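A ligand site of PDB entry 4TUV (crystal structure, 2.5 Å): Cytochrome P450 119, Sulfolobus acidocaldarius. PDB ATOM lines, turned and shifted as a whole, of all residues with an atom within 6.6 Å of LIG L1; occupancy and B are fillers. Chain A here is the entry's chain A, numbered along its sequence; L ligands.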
ATOM      1  N   LEU A  69     -29.086   6.734   4.718  1.00  0.00           N
ATOM      2  CA  LEU A  69     -28.103   6.523   3.665  1.00  0.00           C
ATOM      3  C   LEU A  69     -28.657   6.762   2.243  1.00  0.00           C
ATOM      4  O   LEU A  69     -27.968   7.295   1.375  1.00  0.00           O
ATOM      5  CB  LEU A  69     -27.557   5.095   3.785  1.00  0.00           C
ATOM      6  CG  LEU A  69     -26.407   4.639   2.891  1.00  0.00           C
ATOM      7  CD1 LEU A  69     -25.123   5.435   3.131  1.00  0.00           C
ATOM      8  CD2 LEU A  69     -26.198   3.175   3.180  1.00  0.00           C
ATOM      9  N   VAL A 151     -23.189  -7.426   3.933  1.00  0.00           N
ATOM     10  CA  VAL A 151     -22.988  -6.056   3.473  1.00  0.00           C
ATOM     11  C   VAL A 151     -22.117  -6.069   2.222  1.00  0.00           C
ATOM     12  O   VAL A 151     -20.989  -6.520   2.275  1.00  0.00           O
ATOM     13  CB  VAL A 151     -22.366  -5.187   4.599  1.00  0.00           C
ATOM     14  CG1 VAL A 151     -21.882  -3.871   4.081  1.00  0.00           C
ATOM     15  CG2 VAL A 151     -23.376  -4.957   5.714  1.00  0.00           C
ATOM     16  N   ALA A 152     -22.662  -5.593   1.106  1.00  0.00           N
ATOM     17  CA  ALA A 152     -21.970  -5.702  -0.191  1.00  0.00           C
ATOM     18  C   ALA A 152     -22.604  -4.826  -1.266  1.00  0.00           C
ATOM     19  O   ALA A 152     -23.813  -4.579  -1.248  1.00  0.00           O
ATOM     20  CB  ALA A 152     -21.947  -7.177  -0.671  1.00  0.00           C
ATOM     21  N   PHE A 153     -21.784  -4.342  -2.192  1.00  0.00           N
ATOM     22  CA  PHE A 153     -22.292  -3.731  -3.409  1.00  0.00           C
ATOM     23  C   PHE A 153     -23.233  -4.709  -4.111  1.00  0.00           C
ATOM     24  O   PHE A 153     -22.952  -5.892  -4.231  1.00  0.00           O
ATOM     25  CB  PHE A 153     -21.149  -3.311  -4.324  1.00  0.00           C
ATOM     26  CG  PHE A 153     -21.588  -2.962  -5.737  1.00  0.00           C
ATOM     27  CD1 PHE A 153     -21.499  -3.902  -6.759  1.00  0.00           C
ATOM     28  CD2 PHE A 153     -22.078  -1.698  -6.032  1.00  0.00           C
ATOM     29  CE1 PHE A 153     -21.894  -3.585  -8.046  1.00  0.00           C
ATOM     30  CE2 PHE A 153     -22.474  -1.367  -7.322  1.00  0.00           C
ATOM     31  CZ  PHE A 153     -22.382  -2.319  -8.332  1.00  0.00           C
ATOM     32  N   ARG A 154     -24.364  -4.210  -4.569  1.00  0.00           N
ATOM     33  CA  ARG A 154     -25.338  -5.066  -5.233  1.00  0.00           C
ATOM     34  C   ARG A 154     -25.572  -4.561  -6.639  1.00  0.00           C
ATOM     35  O   ARG A 154     -26.262  -3.567  -6.832  1.00  0.00           O
ATOM     36  CB  ARG A 154     -26.670  -5.094  -4.457  1.00  0.00           C
ATOM     37  CG  ARG A 154     -26.590  -5.565  -3.017  1.00  0.00           C
ATOM     38  CD  ARG A 154     -26.173  -7.056  -2.885  1.00  0.00           C
ATOM     39  NE  ARG A 154     -27.098  -8.038  -3.485  1.00  0.00           N
ATOM     40  CZ  ARG A 154     -28.405  -8.149  -3.222  1.00  0.00           C
ATOM     41  NH1 ARG A 154     -28.998  -7.330  -2.359  1.00  0.00           N
ATOM     42  NH2 ARG A 154     -29.131  -9.093  -3.817  1.00  0.00           N
ATOM     43  N   GLU A 160     -29.003  -0.441  -2.875  1.00  0.00           N
ATOM     44  CA  GLU A 160     -28.946  -1.542  -1.925  1.00  0.00           C
ATOM     45  C   GLU A 160     -27.532  -2.018  -1.574  1.00  0.00           C
ATOM     46  O   GLU A 160     -26.697  -2.195  -2.459  1.00  0.00           O
ATOM     47  CB  GLU A 160     -29.764  -2.721  -2.451  1.00  0.00           C
ATOM     48  CG  GLU A 160     -31.211  -2.393  -2.761  1.00  0.00           C
ATOM     49  CD  GLU A 160     -32.101  -3.617  -2.633  1.00  0.00           C
ATOM     50  OE1 GLU A 160     -31.658  -4.613  -2.000  1.00  0.00           O
ATOM     51  OE2 GLU A 160     -33.242  -3.592  -3.153  1.00  0.00           O
ATOM     52  N   ILE A 161     -27.294  -2.243  -0.288  1.00  0.00           N
ATOM     53  CA  ILE A 161     -25.999  -2.732   0.165  1.00  0.00           C
ATOM     54  C   ILE A 161     -26.075  -3.983   1.067  1.00  0.00           C
ATOM     55  O   ILE A 161     -25.102  -4.362   1.716  1.00  0.00           O
ATOM     56  CB  ILE A 161     -25.226  -1.641   0.906  1.00  0.00           C
ATOM     57  CG1 ILE A 161     -25.935  -1.282   2.217  1.00  0.00           C
ATOM     58  CG2 ILE A 161     -25.075  -0.424   0.012  1.00  0.00           C
ATOM     59  CD1 ILE A 161     -25.165  -0.287   3.022  1.00  0.00           C
ATOM     60  N   LEU A 205     -29.184  -0.973  10.043  1.00  0.00           N
ATOM     61  CA  LEU A 205     -28.129  -0.110   9.553  1.00  0.00           C
ATOM     62  C   LEU A 205     -27.088   0.160  10.628  1.00  0.00           C
ATOM     63  O   LEU A 205     -25.910  -0.105  10.412  1.00  0.00           O
ATOM     64  CB  LEU A 205     -28.715   1.210   9.040  1.00  0.00           C
ATOM     65  CG  LEU A 205     -27.674   2.142   8.410  1.00  0.00           C
ATOM     66  CD1 LEU A 205     -27.252   1.650   7.036  1.00  0.00           C
ATOM     67  CD2 LEU A 205     -28.166   3.562   8.358  1.00  0.00           C
ATOM     68  N   ILE A 208     -25.124  -3.238  11.881  1.00  0.00           N
ATOM     69  CA  ILE A 208     -24.436  -4.178  11.012  1.00  0.00           C
ATOM     70  C   ILE A 208     -23.549  -3.493   9.976  1.00  0.00           C
ATOM     71  O   ILE A 208     -22.472  -3.986   9.641  1.00  0.00           O
ATOM     72  CB  ILE A 208     -25.465  -5.091  10.286  1.00  0.00           C
ATOM     73  CG1 ILE A 208     -26.244  -5.945  11.296  1.00  0.00           C
ATOM     74  CG2 ILE A 208     -24.816  -5.979   9.245  1.00  0.00           C
ATOM     75  CD1 ILE A 208     -25.369  -6.744  12.204  1.00  0.00           C
ATOM     76  N   ALA A 209     -23.997  -2.335   9.482  1.00  0.00           N
ATOM     77  CA  ALA A 209     -23.423  -1.743   8.283  1.00  0.00           C
ATOM     78  C   ALA A 209     -21.993  -1.278   8.468  1.00  0.00           C
ATOM     79  O   ALA A 209     -21.266  -1.180   7.491  1.00  0.00           O
ATOM     80  CB  ALA A 209     -24.253  -0.591   7.824  1.00  0.00           C
ATOM     81  N   GLY A 210     -21.584  -1.027   9.710  1.00  0.00           N
ATOM     82  CA  GLY A 210     -20.272  -0.493   9.999  1.00  0.00           C
ATOM     83  C   GLY A 210     -19.218  -1.517  10.397  1.00  0.00           C
ATOM     84  O   GLY A 210     -18.040  -1.208  10.499  1.00  0.00           O
ATOM     85  N   ASN A 211     -19.647  -2.755  10.619  1.00  0.00           N
ATOM     86  CA  ASN A 211     -18.726  -3.781  11.077  1.00  0.00           C
ATOM     87  C   ASN A 211     -17.581  -4.057  10.109  1.00  0.00           C
ATOM     88  O   ASN A 211     -16.430  -3.782  10.431  1.00  0.00           O
ATOM     89  CB  ASN A 211     -19.518  -5.045  11.397  1.00  0.00           C
ATOM     90  CG  ASN A 211     -20.538  -4.784  12.465  1.00  0.00           C
ATOM     91  OD1 ASN A 211     -20.397  -3.833  13.224  1.00  0.00           O
ATOM     92  ND2 ASN A 211     -21.576  -5.606  12.538  1.00  0.00           N
ATOM     93  N   THR A 213     -16.545  -2.511   7.403  1.00  0.00           N
ATOM     94  CA  THR A 213     -15.750  -1.342   7.011  1.00  0.00           C
ATOM     95  C   THR A 213     -14.714  -1.015   8.084  1.00  0.00           C
ATOM     96  O   THR A 213     -13.547  -0.778   7.769  1.00  0.00           O
ATOM     97  CB  THR A 213     -16.626  -0.090   6.763  1.00  0.00           C
ATOM     98  OG1 THR A 213     -17.424   0.165   7.914  1.00  0.00           O
ATOM     99  CG2 THR A 213     -17.541  -0.292   5.570  1.00  0.00           C
ATOM    100  N   VAL A 254     -14.030   1.933   2.009  1.00  0.00           N
ATOM    101  CA  VAL A 254     -15.060   2.123   0.999  1.00  0.00           C
ATOM    102  C   VAL A 254     -14.437   2.822  -0.201  1.00  0.00           C
ATOM    103  O   VAL A 254     -13.967   3.943  -0.089  1.00  0.00           O
ATOM    104  CB  VAL A 254     -16.262   2.919   1.549  1.00  0.00           C
ATOM    105  CG1 VAL A 254     -17.380   3.032   0.496  1.00  0.00           C
ATOM    106  CG2 VAL A 254     -16.786   2.250   2.800  1.00  0.00           C
ATOM    107  N   ARG A 256     -15.679   3.782  -3.109  1.00  0.00           N
ATOM    108  CA  ARG A 256     -16.489   4.617  -3.953  1.00  0.00           C
ATOM    109  C   ARG A 256     -17.929   4.676  -3.452  1.00  0.00           C
ATOM    110  O   ARG A 256     -18.351   3.883  -2.611  1.00  0.00           O
ATOM    111  CB  ARG A 256     -16.479   4.106  -5.399  1.00  0.00           C
ATOM    112  CG  ARG A 256     -17.384   2.921  -5.610  1.00  0.00           C
ATOM    113  CD  ARG A 256     -17.345   2.400  -7.017  1.00  0.00           C
ATOM    114  NE  ARG A 256     -18.388   1.396  -7.200  1.00  0.00           N
ATOM    115  CZ  ARG A 256     -18.250   0.284  -7.908  1.00  0.00           C
ATOM    116  NH1 ARG A 256     -17.107   0.013  -8.524  1.00  0.00           N
ATOM    117  NH2 ARG A 256     -19.255  -0.574  -8.007  1.00  0.00           N
ATOM    118  N   THR A 257     -18.671   5.646  -3.984  1.00  0.00           N
ATOM    119  CA  THR A 257     -20.064   5.780  -3.695  1.00  0.00           C
ATOM    120  C   THR A 257     -20.737   6.278  -4.975  1.00  0.00           C
ATOM    121  O   THR A 257     -20.057   6.585  -5.965  1.00  0.00           O
ATOM    122  CB  THR A 257     -20.306   6.734  -2.499  1.00  0.00           C
ATOM    123  OG1 THR A 257     -21.658   6.613  -2.030  1.00  0.00           O
ATOM    124  CG2 THR A 257     -20.084   8.133  -2.906  1.00  0.00           C
ATOM    125  N   CYS A 317     -19.907  10.054   7.008  1.00  0.00           N
ATOM    126  CA  CYS A 317     -20.121   8.849   7.825  1.00  0.00           C
ATOM    127  C   CYS A 317     -20.468   9.123   9.293  1.00  0.00           C
ATOM    128  O   CYS A 317     -19.691   9.729  10.045  1.00  0.00           O
ATOM    129  CB  CYS A 317     -18.906   7.944   7.756  1.00  0.00           C
ATOM    130  SG  CYS A 317     -19.062   6.462   8.807  1.00  0.00           S
ATOM    131  N   LEU A 318     -21.643   8.660   9.673  1.00  0.00           N
ATOM    132  CA  LEU A 318     -22.109   8.719  11.053  1.00  0.00           C
ATOM    133  C   LEU A 318     -21.163   7.978  11.990  1.00  0.00           C
ATOM    134  O   LEU A 318     -21.022   8.354  13.146  1.00  0.00           O
ATOM    135  CB  LEU A 318     -23.520   8.137  11.153  1.00  0.00           C
ATOM    136  CG  LEU A 318     -24.213   8.186  12.505  1.00  0.00           C
ATOM    137  CD1 LEU A 318     -24.318   9.625  12.996  1.00  0.00           C
ATOM    138  CD2 LEU A 318     -25.615   7.510  12.440  1.00  0.00           C
ATOM    139  N   GLY A 319     -20.513   6.921  11.497  1.00  0.00           N
ATOM    140  CA  GLY A 319     -19.617   6.127  12.318  1.00  0.00           C
ATOM    141  C   GLY A 319     -18.169   6.588  12.346  1.00  0.00           C
ATOM    142  O   GLY A 319     -17.319   5.945  12.951  1.00  0.00           O
ATOM    143  N   VAL A 353     -16.552  -2.584  -4.016  1.00  0.00           N
ATOM    144  CA  VAL A 353     -16.644  -1.363  -3.236  1.00  0.00           C
ATOM    145  C   VAL A 353     -15.888  -1.474  -1.926  1.00  0.00           C
ATOM    146  O   VAL A 353     -15.102  -0.599  -1.572  1.00  0.00           O
ATOM    147  CB  VAL A 353     -18.126  -0.977  -2.974  1.00  0.00           C
ATOM    148  CG1 VAL A 353     -18.208   0.146  -1.955  1.00  0.00           C
ATOM    149  CG2 VAL A 353     -18.824  -0.588  -4.277  1.00  0.00           C
ATOM    150  N   LEU A 354     -16.134  -2.565  -1.205  1.00  0.00           N
ATOM    151  CA  LEU A 354     -15.438  -2.847   0.052  1.00  0.00           C
ATOM    152  C   LEU A 354     -14.002  -3.304  -0.176  1.00  0.00           C
ATOM    153  O   LEU A 354     -13.717  -4.165  -1.007  1.00  0.00           O
ATOM    154  CB  LEU A 354     -16.203  -3.907   0.818  1.00  0.00           C
ATOM    155  CG  LEU A 354     -17.520  -3.335   1.303  1.00  0.00           C
ATOM    156  CD1 LEU A 354     -18.409  -4.434   1.858  1.00  0.00           C
ATOM    157  CD2 LEU A 354     -17.261  -2.268   2.360  1.00  0.00           C
HETATM  158  C1  LIG L   1     -20.726   1.621   2.334  1.00  0.00           C
HETATM  159  C2  LIG L   1     -20.826   0.927   1.103  1.00  0.00           C
HETATM  160  C3  LIG L   1     -21.003  -0.445   1.124  1.00  0.00           C
HETATM  161  C4  LIG L   1     -21.065  -1.152   2.329  1.00  0.00           C
HETATM  162  C5  LIG L   1     -20.968  -0.462   3.541  1.00  0.00           C
HETATM  163  C6  LIG L   1     -20.803   0.910   3.532  1.00  0.00           C
HETATM  164  C7  LIG L   1     -20.693   1.635   4.796  1.00  0.00           C
HETATM  165  C8  LIG L   1     -20.385   2.965   5.078  1.00  0.00           C
HETATM  166  N1  LIG L   1     -20.412   3.213   6.465  1.00  0.00           N
HETATM  167  C9  LIG L   1     -20.734   2.001   7.008  1.00  0.00           C
HETATM  168  N2  LIG L   1     -20.901   1.036   6.038  1.00  0.00           N
HETATM  169 CL1  LIG L   1     -21.125  -1.313  -0.416  1.00  0.00          CL
HETATM  170  C1  LG2 L   2     -17.361   5.025   5.134  1.00  0.00           C
HETATM  171  C2  LG2 L   2     -17.684   3.071   9.539  1.00  0.00           C
HETATM  172  C3  LG2 L   2     -22.413   3.982   9.417  1.00  0.00           C
HETATM  173  C4  LG2 L   2     -20.566   6.534   4.996  1.00  0.00           C
HETATM  174  C5  LG2 L   2     -19.980   7.028   3.778  1.00  0.00           C
HETATM  175  C6  LG2 L   2     -18.754   6.531   3.704  1.00  0.00           C
HETATM  176  C7  LG2 L   2     -18.532   5.693   4.869  1.00  0.00           C
HETATM  177  C8  LG2 L   2     -17.730   6.760   2.581  1.00  0.00           C
HETATM  178  C9  LG2 L   2     -20.667   7.971   2.767  1.00  0.00           C
HETATM  179  C10 LG2 L   2     -21.724   7.223   1.944  1.00  0.00           C
HETATM  180  C11 LG2 L   2     -22.364   8.179   0.964  1.00  0.00           C
HETATM  181  O1  LG2 L   2     -22.020   9.390   0.958  1.00  0.00           O
HETATM  182  O2  LG2 L   2     -23.219   7.726   0.156  1.00  0.00           O
HETATM  183  C12 LG2 L   2     -17.038   4.391   6.309  1.00  0.00           C
HETATM  184  C13 LG2 L   2     -15.725   3.868   6.633  1.00  0.00           C
HETATM  185  C14 LG2 L   2     -15.832   3.311   7.850  1.00  0.00           C
HETATM  186  C15 LG2 L   2     -17.192   3.482   8.323  1.00  0.00           C
HETATM  187  C16 LG2 L   2     -14.494   3.952   5.702  1.00  0.00           C
HETATM  188  C17 LG2 L   2     -14.746   2.626   8.701  1.00  0.00           C
HETATM  189  C18 LG2 L   2     -13.430   2.748   8.455  1.00  0.00           C
HETATM  190  C19 LG2 L   2     -18.997   3.182   9.916  1.00  0.00           C
HETATM  191  C20 LG2 L   2     -19.574   2.782  11.193  1.00  0.00           C
HETATM  192  C21 LG2 L   2     -20.892   3.063  11.125  1.00  0.00           C
HETATM  193  C22 LG2 L   2     -21.170   3.600   9.821  1.00  0.00           C
HETATM  194  C23 LG2 L   2     -18.790   2.192  12.396  1.00  0.00           C
HETATM  195  C24 LG2 L   2     -22.036   2.853  12.135  1.00  0.00           C
HETATM  196  C25 LG2 L   2     -21.999   2.036  13.187  1.00  0.00           C
HETATM  197  C26 LG2 L   2     -22.741   4.876   8.430  1.00  0.00           C
HETATM  198  C27 LG2 L   2     -24.020   5.515   8.281  1.00  0.00           C
HETATM  199  C28 LG2 L   2     -23.952   6.302   7.201  1.00  0.00           C
HETATM  200  C29 LG2 L   2     -22.631   6.173   6.641  1.00  0.00           C
HETATM  201  C30 LG2 L   2     -25.263   5.352   9.191  1.00  0.00           C
HETATM  202  C31 LG2 L   2     -25.045   7.189   6.634  1.00  0.00           C
HETATM  203  C32 LG2 L   2     -24.794   8.618   7.097  1.00  0.00           C
HETATM  204  C33 LG2 L   2     -25.802   9.540   6.448  1.00  0.00           C
HETATM  205  O3  LG2 L   2     -26.518   9.123   5.497  1.00  0.00           O
HETATM  206  O4  LG2 L   2     -25.892  10.723   6.863  1.00  0.00           O
HETATM  207  N1  LG2 L   2     -19.665   5.719   5.656  1.00  0.00           N
HETATM  208  N2  LG2 L   2     -17.910   4.151   7.340  1.00  0.00           N
HETATM  209  N3  LG2 L   2     -20.006   3.664   9.092  1.00  0.00           N
HETATM  210  N4  LG2 L   2     -21.902   5.281   7.405  1.00  0.00           N
HETATM  211 FE1  LG2 L   2     -19.861   4.745   7.463  1.00  0.00          FE
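Val 151 touches LIG L1 (CG1 to C4, 3.3 Å).
Ala 152 touches LIG L1.
N of Phe 153 touches CL1 of LIG L1, 3.6 Å away.
Gly 210 touches LIG L1 (CA to C9, 3.9 Å).
CG2 of Thr 213 touches N2 of LIG L1, 3.6 Å away.
Val 353 touches LIG L1 (CG1 to CL1, 3.6 Å).
CD2 of Leu 354 touches C4 of LIG L1, at 3.96 Å.
Within 4 Å of LIG L1: Val 151, Ala 152, Phe 153, Ala 209, Gly 210, Thr 213, Val 353 and Leu 354.
OG1 of Thr 213 sits at hydrogen-bond distance from O of Gly 210, at 3.0 Å.
O of Ile 161 lies within hydrogen-bond range of N of Ala 152 (2.8 Å).
A nitrogen (N1) of LIG L1 is bound to an iron atom (FE1) of LG2 L2.
The backbone carbonyl oxygen (O) of Ala 209 sits at hydrogen-bond distance from a nitrogen (N2) of LIG L1 (2.7 Å).
The side-chain sulfur (SG) of Cys 317 binds an iron atom (FE1) of LG2 L2, at 2.3 Å.
The side-chain hydroxyl of Thr 257 sits at hydrogen-bond distance from an oxygen (O2) of LG2 L2 (2.9 Å).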
